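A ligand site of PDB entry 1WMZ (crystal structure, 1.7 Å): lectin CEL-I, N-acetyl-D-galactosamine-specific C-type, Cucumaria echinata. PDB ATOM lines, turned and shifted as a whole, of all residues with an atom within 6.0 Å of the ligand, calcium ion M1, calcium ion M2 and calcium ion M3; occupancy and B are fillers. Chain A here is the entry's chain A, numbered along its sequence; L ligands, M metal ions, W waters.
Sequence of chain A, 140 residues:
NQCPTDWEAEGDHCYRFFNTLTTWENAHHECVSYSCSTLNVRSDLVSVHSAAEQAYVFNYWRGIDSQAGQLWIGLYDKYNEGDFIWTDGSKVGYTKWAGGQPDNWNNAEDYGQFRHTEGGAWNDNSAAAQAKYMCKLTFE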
ATOM      1  N   GLN A  70      -9.904   2.168   1.579  1.00  0.00           N
ATOM      2  CA  GLN A  70     -10.055   3.539   1.095  1.00  0.00           C
ATOM      3  C   GLN A  70     -11.446   4.123   1.410  1.00  0.00           C
ATOM      4  O   GLN A  70     -12.363   3.399   1.790  1.00  0.00           O
ATOM      5  CB  GLN A  70      -9.821   3.558  -0.408  1.00  0.00           C
ATOM      6  CG  GLN A  70      -8.329   3.266  -0.740  1.00  0.00           C
ATOM      7  CD  GLN A  70      -8.011   1.759  -0.755  1.00  0.00           C
ATOM      8  OE1 GLN A  70      -8.623   0.987  -1.470  1.00  0.00           O
ATOM      9  NE2 GLN A  70      -7.014   1.369   0.011  1.00  0.00           N
ATOM     10  N   ASP A  77     -12.595  12.754 -12.608  1.00  0.00           N
ATOM     11  CA  ASP A  77     -12.180  13.282 -13.905  1.00  0.00           C
ATOM     12  C   ASP A  77     -12.795  12.460 -15.054  1.00  0.00           C
ATOM     13  O   ASP A  77     -12.216  12.360 -16.142  1.00  0.00           O
ATOM     14  CB  ASP A  77     -10.652  13.347 -14.003  1.00  0.00           C
ATOM     15  CG  ASP A  77     -10.022  12.021 -14.361  1.00  0.00           C
ATOM     16  OD1 ASP A  77     -10.573  10.954 -13.997  1.00  0.00           O
ATOM     17  OD2 ASP A  77      -8.961  11.952 -15.035  1.00  0.00           O
ATOM     18  N   LYS A  78     -13.975  11.889 -14.811  1.00  0.00           N
ATOM     19  CA  LYS A  78     -14.727  11.098 -15.803  1.00  0.00           C
ATOM     20  C   LYS A  78     -15.032  11.891 -17.074  1.00  0.00           C
ATOM     21  O   LYS A  78     -14.890  11.360 -18.193  1.00  0.00           O
ATOM     22  CB  LYS A  78     -16.058  10.626 -15.205  1.00  0.00           C
ATOM     23  CG  LYS A  78     -16.872   9.706 -16.118  1.00  0.00           C
ATOM     24  CD  LYS A  78     -18.351   9.968 -15.938  1.00  0.00           C
ATOM     25  CE  LYS A  78     -19.230   9.003 -16.737  1.00  0.00           C
ATOM     26  NZ  LYS A  78     -19.724   7.829 -15.914  1.00  0.00           N
ATOM     27  N   GLU A  81     -10.641  13.757 -18.903  1.00  0.00           N
ATOM     28  CA  GLU A  81      -9.446  13.066 -18.382  1.00  0.00           C
ATOM     29  C   GLU A  81      -8.342  14.024 -17.972  1.00  0.00           C
ATOM     30  O   GLU A  81      -7.913  14.896 -18.757  1.00  0.00           O
ATOM     31  CB  GLU A  81      -8.931  12.049 -19.401  1.00  0.00           C
ATOM     32  CG  GLU A  81      -7.728  11.204 -18.909  1.00  0.00           C
ATOM     33  CD  GLU A  81      -7.950  10.472 -17.584  1.00  0.00           C
ATOM     34  OE1 GLU A  81      -7.031  10.447 -16.751  1.00  0.00           O
ATOM     35  OE2 GLU A  81      -9.034   9.905 -17.390  1.00  0.00           O
ATOM     36  N   GLY A  82      -7.902  13.857 -16.719  1.00  0.00           N
ATOM     37  CA  GLY A  82      -6.867  14.652 -16.095  1.00  0.00           C
ATOM     38  C   GLY A  82      -7.288  15.905 -15.368  1.00  0.00           C
ATOM     39  O   GLY A  82      -6.504  16.461 -14.616  1.00  0.00           O
ATOM     40  N   PHE A  84      -9.507  17.033 -12.622  1.00  0.00           N
ATOM     41  CA  PHE A  84     -10.283  16.582 -11.462  1.00  0.00           C
ATOM     42  C   PHE A  84     -11.152  17.713 -10.941  1.00  0.00           C
ATOM     43  O   PHE A  84     -10.684  18.866 -10.817  1.00  0.00           O
ATOM     44  CB  PHE A  84      -9.375  15.984 -10.395  1.00  0.00           C
ATOM     45  CG  PHE A  84      -8.986  14.559 -10.709  1.00  0.00           C
ATOM     46  CD1 PHE A  84      -9.803  13.516 -10.323  1.00  0.00           C
ATOM     47  CD2 PHE A  84      -7.812  14.289 -11.425  1.00  0.00           C
ATOM     48  CE1 PHE A  84      -9.492  12.214 -10.591  1.00  0.00           C
ATOM     49  CE2 PHE A  84      -7.472  12.969 -11.716  1.00  0.00           C
ATOM     50  CZ  PHE A  84      -8.313  11.921 -11.314  1.00  0.00           C
ATOM     51  N   GLY A 100       2.970   9.770  -6.639  1.00  0.00           N
ATOM     52  CA  GLY A 100       2.718   8.954  -7.837  1.00  0.00           C
ATOM     53  C   GLY A 100       1.291   8.991  -8.365  1.00  0.00           C
ATOM     54  O   GLY A 100       0.969   8.310  -9.360  1.00  0.00           O
ATOM     55  N   GLN A 101       0.459   9.802  -7.700  1.00  0.00           N
ATOM     56  CA  GLN A 101      -0.972   9.930  -8.027  1.00  0.00           C
ATOM     57  C   GLN A 101      -1.319  11.388  -8.357  1.00  0.00           C
ATOM     58  O   GLN A 101      -0.677  12.317  -7.837  1.00  0.00           O
ATOM     59  CB  GLN A 101      -1.805   9.484  -6.807  1.00  0.00           C
ATOM     60  CG  GLN A 101      -1.507   8.069  -6.319  1.00  0.00           C
ATOM     61  CD  GLN A 101      -1.737   6.992  -7.358  1.00  0.00           C
ATOM     62  OE1 GLN A 101      -2.436   7.187  -8.316  1.00  0.00           O
ATOM     63  NE2 GLN A 101      -1.091   5.841  -7.176  1.00  0.00           N
ATOM     64  N   PRO A 102      -2.319  11.620  -9.191  1.00  0.00           N
ATOM     65  CA  PRO A 102      -3.124  10.602  -9.881  1.00  0.00           C
ATOM     66  C   PRO A 102      -2.377  10.062 -11.098  1.00  0.00           C
ATOM     67  O   PRO A 102      -1.538  10.763 -11.666  1.00  0.00           O
ATOM     68  CB  PRO A 102      -4.346  11.413 -10.357  1.00  0.00           C
ATOM     69  CG  PRO A 102      -3.794  12.736 -10.646  1.00  0.00           C
ATOM     70  CD  PRO A 102      -2.732  12.972  -9.610  1.00  0.00           C
ATOM     71  N   ASP A 103      -2.685   8.856 -11.500  1.00  0.00           N
ATOM     72  CA  ASP A 103      -1.931   8.160 -12.571  1.00  0.00           C
ATOM     73  C   ASP A 103      -2.788   7.514 -13.639  1.00  0.00           C
ATOM     74  O   ASP A 103      -2.272   6.912 -14.552  1.00  0.00           O
ATOM     75  CB  ASP A 103      -0.942   7.138 -11.961  1.00  0.00           C
ATOM     76  CG  ASP A 103      -1.646   6.002 -11.253  1.00  0.00           C
ATOM     77  OD1 ASP A 103      -0.968   4.990 -10.851  1.00  0.00           O
ATOM     78  OD2 ASP A 103      -2.886   6.022 -11.035  1.00  0.00           O
ATOM     79  N   ASN A 104      -4.107   7.623 -13.552  1.00  0.00           N
ATOM     80  CA  ASN A 104      -5.012   7.000 -14.506  1.00  0.00           C
ATOM     81  C   ASN A 104      -4.611   5.561 -14.876  1.00  0.00           C
ATOM     82  O   ASN A 104      -4.594   5.191 -16.039  1.00  0.00           O
ATOM     83  CB  ASN A 104      -5.119   7.880 -15.767  1.00  0.00           C
ATOM     84  CG  ASN A 104      -6.353   7.585 -16.580  1.00  0.00           C
ATOM     85  OD1 ASN A 104      -7.481   7.484 -16.063  1.00  0.00           O
ATOM     86  ND2 ASN A 104      -6.161   7.482 -17.881  1.00  0.00           N
ATOM     87  N   TRP A 105      -4.293   4.769 -13.865  1.00  0.00           N
ATOM     88  CA  TRP A 105      -3.788   3.429 -14.094  1.00  0.00           C
ATOM     89  C   TRP A 105      -4.736   2.630 -14.975  1.00  0.00           C
ATOM     90  O   TRP A 105      -5.953   2.620 -14.774  1.00  0.00           O
ATOM     91  CB  TRP A 105      -3.596   2.758 -12.742  1.00  0.00           C
ATOM     92  CG  TRP A 105      -2.944   1.443 -12.773  1.00  0.00           C
ATOM     93  CD1 TRP A 105      -1.653   1.178 -13.015  1.00  0.00           C
ATOM     94  CD2 TRP A 105      -3.569   0.186 -12.461  1.00  0.00           C
ATOM     95  NE1 TRP A 105      -1.401  -0.163 -12.869  1.00  0.00           N
ATOM     96  CE2 TRP A 105      -2.572  -0.797 -12.562  1.00  0.00           C
ATOM     97  CE3 TRP A 105      -4.868  -0.210 -12.143  1.00  0.00           C
ATOM     98  CZ2 TRP A 105      -2.833  -2.149 -12.333  1.00  0.00           C
ATOM     99  CZ3 TRP A 105      -5.137  -1.550 -11.915  1.00  0.00           C
ATOM    100  CH2 TRP A 105      -4.114  -2.510 -12.030  1.00  0.00           C
ATOM    101  N   ASN A 107      -5.727   3.289 -17.723  1.00  0.00           N
ATOM    102  CA  ASN A 107      -6.673   4.224 -18.378  1.00  0.00           C
ATOM    103  C   ASN A 107      -8.096   4.152 -17.868  1.00  0.00           C
ATOM    104  O   ASN A 107      -9.018   4.510 -18.573  1.00  0.00           O
ATOM    105  CB  ASN A 107      -6.655   3.989 -19.884  1.00  0.00           C
ATOM    106  CG  ASN A 107      -5.274   4.127 -20.474  1.00  0.00           C
ATOM    107  OD1 ASN A 107      -4.643   5.210 -20.385  1.00  0.00           O
ATOM    108  ND2 ASN A 107      -4.779   3.060 -21.098  1.00  0.00           N
ATOM    109  N   ALA A 108      -8.286   3.755 -16.625  1.00  0.00           N
ATOM    110  CA  ALA A 108      -9.625   3.503 -16.104  1.00  0.00           C
ATOM    111  C   ALA A 108      -9.866   4.083 -14.700  1.00  0.00           C
ATOM    112  O   ALA A 108     -10.882   3.763 -14.052  1.00  0.00           O
ATOM    113  CB  ALA A 108      -9.913   2.037 -16.129  1.00  0.00           C
ATOM    114  N   GLU A 109      -8.959   4.936 -14.221  1.00  0.00           N
ATOM    115  CA  GLU A 109      -9.100   5.510 -12.902  1.00  0.00           C
ATOM    116  C   GLU A 109      -9.516   7.000 -12.970  1.00  0.00           C
ATOM    117  O   GLU A 109      -8.699   7.882 -13.307  1.00  0.00           O
ATOM    118  CB  GLU A 109      -7.822   5.337 -12.061  1.00  0.00           C
ATOM    119  CG  GLU A 109      -7.332   3.894 -11.971  1.00  0.00           C
ATOM    120  CD  GLU A 109      -6.302   3.708 -10.916  1.00  0.00           C
ATOM    121  OE1 GLU A 109      -5.437   4.591 -10.737  1.00  0.00           O
ATOM    122  OE2 GLU A 109      -6.325   2.650 -10.209  1.00  0.00           O
ATOM    123  N   ASP A 110     -10.772   7.247 -12.604  1.00  0.00           N
ATOM    124  CA  ASP A 110     -11.393   8.591 -12.652  1.00  0.00           C
ATOM    125  C   ASP A 110     -12.074   9.046 -11.350  1.00  0.00           C
ATOM    126  O   ASP A 110     -12.759  10.058 -11.345  1.00  0.00           O
ATOM    127  CB  ASP A 110     -12.453   8.624 -13.738  1.00  0.00           C
ATOM    128  CG  ASP A 110     -11.990   8.003 -15.060  1.00  0.00           C
ATOM    129  OD1 ASP A 110     -12.809   7.275 -15.656  1.00  0.00           O
ATOM    130  OD2 ASP A 110     -10.863   8.168 -15.588  1.00  0.00           O
ATOM    131  N   TYR A 111     -11.906   8.310 -10.278  1.00  0.00           N
ATOM    132  CA  TYR A 111     -12.685   8.492  -9.053  1.00  0.00           C
ATOM    133  C   TYR A 111     -11.762   8.603  -7.846  1.00  0.00           C
ATOM    134  O   TYR A 111     -10.974   7.707  -7.534  1.00  0.00           O
ATOM    135  CB  TYR A 111     -13.661   7.287  -8.942  1.00  0.00           C
ATOM    136  CG  TYR A 111     -14.448   7.104 -10.206  1.00  0.00           C
ATOM    137  CD1 TYR A 111     -14.184   6.039 -11.092  1.00  0.00           C
ATOM    138  CD2 TYR A 111     -15.392   8.042 -10.577  1.00  0.00           C
ATOM    139  CE1 TYR A 111     -14.911   5.899 -12.281  1.00  0.00           C
ATOM    140  CE2 TYR A 111     -16.111   7.917 -11.741  1.00  0.00           C
ATOM    141  CZ  TYR A 111     -15.871   6.840 -12.604  1.00  0.00           C
ATOM    142  OH  TYR A 111     -16.563   6.755 -13.781  1.00  0.00           O
ATOM    143  N   GLN A 113     -10.364   9.168  -3.897  1.00  0.00           N
ATOM    144  CA  GLN A 113     -10.534   8.471  -2.622  1.00  0.00           C
ATOM    145  C   GLN A 113      -9.327   8.732  -1.723  1.00  0.00           C
ATOM    146  O   GLN A 113      -8.195   8.912  -2.212  1.00  0.00           O
ATOM    147  CB  GLN A 113     -10.714   6.967  -2.856  1.00  0.00           C
ATOM    148  CG  GLN A 113      -9.484   6.324  -3.587  1.00  0.00           C
ATOM    149  CD  GLN A 113      -9.510   4.761  -3.764  1.00  0.00           C
ATOM    150  OE1 GLN A 113      -8.437   4.167  -4.006  1.00  0.00           O
ATOM    151  NE2 GLN A 113     -10.681   4.146  -3.711  1.00  0.00           N
ATOM    152  N   ARG A 115      -6.643   7.217   0.798  1.00  0.00           N
ATOM    153  CA  ARG A 115      -6.006   6.069   1.431  1.00  0.00           C
ATOM    154  C   ARG A 115      -6.175   6.073   2.951  1.00  0.00           C
ATOM    155  O   ARG A 115      -6.425   7.128   3.555  1.00  0.00           O
ATOM    156  CB  ARG A 115      -4.522   6.054   1.113  1.00  0.00           C
ATOM    157  CG  ARG A 115      -4.211   5.748  -0.287  1.00  0.00           C
ATOM    158  CD  ARG A 115      -2.751   5.837  -0.576  1.00  0.00           C
ATOM    159  NE  ARG A 115      -2.430   5.353  -1.918  1.00  0.00           N
ATOM    160  CZ  ARG A 115      -1.230   5.470  -2.466  1.00  0.00           C
ATOM    161  NH1 ARG A 115      -0.238   6.061  -1.791  1.00  0.00           N
ATOM    162  NH2 ARG A 115      -1.035   5.060  -3.697  1.00  0.00           N
ATOM    163  N   ASN A 123      -5.870   9.094  -3.915  1.00  0.00           N
ATOM    164  CA  ASN A 123      -5.627   8.217  -5.051  1.00  0.00           C
ATOM    165  C   ASN A 123      -6.803   8.300  -6.010  1.00  0.00           C
ATOM    166  O   ASN A 123      -7.956   8.447  -5.609  1.00  0.00           O
ATOM    167  CB  ASN A 123      -5.495   6.774  -4.598  1.00  0.00           C
ATOM    168  CG  ASN A 123      -5.401   5.831  -5.752  1.00  0.00           C
ATOM    169  OD1 ASN A 123      -4.509   5.999  -6.608  1.00  0.00           O
ATOM    170  ND2 ASN A 123      -6.277   4.812  -5.803  1.00  0.00           N
ATOM    171  N   ASP A 124      -6.528   8.181  -7.306  1.00  0.00           N
ATOM    172  CA  ASP A 124      -7.593   7.926  -8.249  1.00  0.00           C
ATOM    173  C   ASP A 124      -7.756   6.450  -8.477  1.00  0.00           C
ATOM    174  O   ASP A 124      -6.757   5.751  -8.656  1.00  0.00           O
ATOM    175  CB  ASP A 124      -7.354   8.658  -9.593  1.00  0.00           C
ATOM    176  CG  ASP A 124      -6.041   8.278 -10.251  1.00  0.00           C
ATOM    177  OD1 ASP A 124      -5.099   7.849  -9.546  1.00  0.00           O
ATOM    178  OD2 ASP A 124      -5.869   8.443 -11.476  1.00  0.00           O
ATOM    179  N   ASN A 125      -8.993   5.947  -8.486  1.00  0.00           N
ATOM    180  CA  ASN A 125      -9.287   4.535  -8.691  1.00  0.00           C
ATOM    181  C   ASN A 125     -10.458   4.343  -9.702  1.00  0.00           C
ATOM    182  O   ASN A 125     -11.023   5.315 -10.195  1.00  0.00           O
ATOM    183  CB  ASN A 125      -9.566   3.889  -7.317  1.00  0.00           C
ATOM    184  CG  ASN A 125      -9.105   2.436  -7.227  1.00  0.00           C
ATOM    185  OD1 ASN A 125      -9.251   1.673  -8.191  1.00  0.00           O
ATOM    186  ND2 ASN A 125      -8.632   2.055  -6.088  1.00  0.00           N
HETATM  187  C1  LIG L   1      -1.898   1.991  -6.059  1.00  0.00           C
HETATM  188  C2  LIG L   1      -3.308   2.566  -6.340  1.00  0.00           C
HETATM  189  C3  LIG L   1      -3.905   2.462  -7.721  1.00  0.00           C
HETATM  190  C4  LIG L   1      -2.886   2.419  -8.820  1.00  0.00           C
HETATM  191  C5  LIG L   1      -1.544   1.805  -8.514  1.00  0.00           C
HETATM  192  C6  LIG L   1      -0.473   2.043  -9.599  1.00  0.00           C
HETATM  193  C7  LIG L   1      -4.430   2.883  -4.207  1.00  0.00           C
HETATM  194  C8  LIG L   1      -5.484   2.342  -3.282  1.00  0.00           C
HETATM  195  N1  LIG L   1      -4.270   2.196  -5.345  1.00  0.00           N
HETATM  196  O1  LIG L   1      -1.223   2.526  -4.919  1.00  0.00           O
HETATM  197  O2  LIG L   1      -4.986   3.346  -8.048  1.00  0.00           O
HETATM  198  O3  LIG L   1      -2.533   3.801  -8.966  1.00  0.00           O
HETATM  199  O4  LIG L   1      -1.019   1.943  -7.208  1.00  0.00           O
HETATM  200  O5  LIG L   1       0.548   1.088  -9.290  1.00  0.00           O
HETATM  201  O6  LIG L   1      -3.787   3.888  -3.945  1.00  0.00           O
HETATM  202 CA    CA M   1      -8.672   9.545 -15.014  1.00  0.00          CA
HETATM  203 CA    CA M   2      -4.335   5.580  -9.070  1.00  0.00          CA
HETATM  204 CA    CA M   3     -11.206   8.651 -17.915  1.00  0.00          CA
HETATM  205  O   HOH W   1       2.826   1.363 -10.562  1.00  0.00           O
HETATM  206  O   HOH W   2     -11.934  10.733 -18.238  1.00  0.00           O
HETATM  207  O   HOH W   3      -0.420  -1.464  -9.569  1.00  0.00           O
HETATM  208  O   HOH W   4      -6.770   9.841 -13.605  1.00  0.00           O
HETATM  209  O   HOH W   5      -5.975  -0.248  -5.662  1.00  0.00           O
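Within 4 Å of calcium ion M1: Asp 77, Glu 81, Asn 104, Glu 109 and Asp 110.
Of the 22 residues printed, 5 come within 4 Å of calcium ion M2. The nearest printed residue that does not touch calcium ion M2 is Trp 105 (4.7 Å).
NH2 of Arg 115 lies within hydrogen-bond range of O1 of the ligand, at 2.8 Å.
Water W4 lies within hydrogen-bond range of the side-chain carboxylate (OD2) of Asp 124 (2.7 Å) and the backbone NH (N) of Asn 104 (3.5 Å).
O of Glu 109 binds calcium ion M1, at 2.4 Å. Water W4 is bound to calcium ion M1 (2.4 Å). Calcium ion M1 is bound by OD2 of Asp 77, at 2.4 Å. OE2 of Glu 81 binds calcium ion M1 (2.4 Å). Calcium ion M1 is bound by OE1 of Glu 81 (2.6 Å). OD1 of Asp 77 is bound to calcium ion M1 (2.6 Å). Calcium ion M1 is bound by the side-chain amide oxygen (OD1) of Asn 104 (2.6 Å). OD2 of Asp 110 binds calcium ion M1, at 2.7 Å. Calcium ion M1 has eight donor atoms within binding distance.
CD of Gln 70 touches C8 of the ligand, at 3.6 Å. Trp 105 touches the ligand (CD1 to C6, 3.7 Å). OE1 of Gln 113 touches C8 of the ligand, 3.5 Å away. Hydrophobic or aromatic side chains that line the ligand: Trp 105. Within 4 Å of the ligand: Gln 70, Gln 101, Asp 103, Trp 105, Glu 109, Gln 113, Arg 115, Asn 123 and Asp 124. The nearest printed residue that does not touch the ligand is Asn 125 (4.2 Å).
Calcium ion M3 is bound by water W2 (2.2 Å), the side-chain carboxylate of Asp 110 (2.4 Å) and the side-chain carboxylate of Glu 81 (2.6 Å). Calcium ion M3 has three donor atoms within binding distance. Slightly farther from calcium ion M3 lies OD1 of Asp 110 (3.1 Å).
OE1 of Glu 109 sits close to N of Trp 105. The backbone carbonyl oxygen (O) of Asn 125 lies within hydrogen-bond range of the backbone NH (N) of Asp 110, at 3.1 Å. The backbone NH of Gly 82 lies close to the side-chain carboxylate of Asp 77 (2.8 Å). The side-chain carboxylate of Asp 124 sits at hydrogen-bond distance from the backbone NH of Asn 104, at 2.8 Å. The side-chain carboxylate (OD2) of Asp 103 lies close to the backbone NH (N) of Trp 105. ND2 of Asn 123 sits at hydrogen-bond distance from OE1 of Gln 113. The side-chain amide oxygen (OE1) of Gln 113 lies within hydrogen-bond range of the side-chain amide nitrogen (ND2) of Asn 125 (3.0 Å).
Calcium ion M2 is bound by OE1 of Glu 109. The side-chain carboxylate (OD1) of Asp 124 is bound to calcium ion M2 (2.4 Å). Calcium ion M2 is bound by O of Asp 124 (2.5 Å). The side-chain carboxylate (OD2) of Asp 103 is bound to calcium ion M2. The side-chain amide oxygen (OD1) of Asn 123 is bound to calcium ion M2. Calcium ion M2 is bound by an oxygen (O3) of the ligand, 2.5 Å away. Calcium ion M2 is bound by O2 of the ligand. The side-chain amide oxygen (OE1) of Gln 101 is bound to calcium ion M2 (2.6 Å). Calcium ion M2 has eight donor atoms within binding distance.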
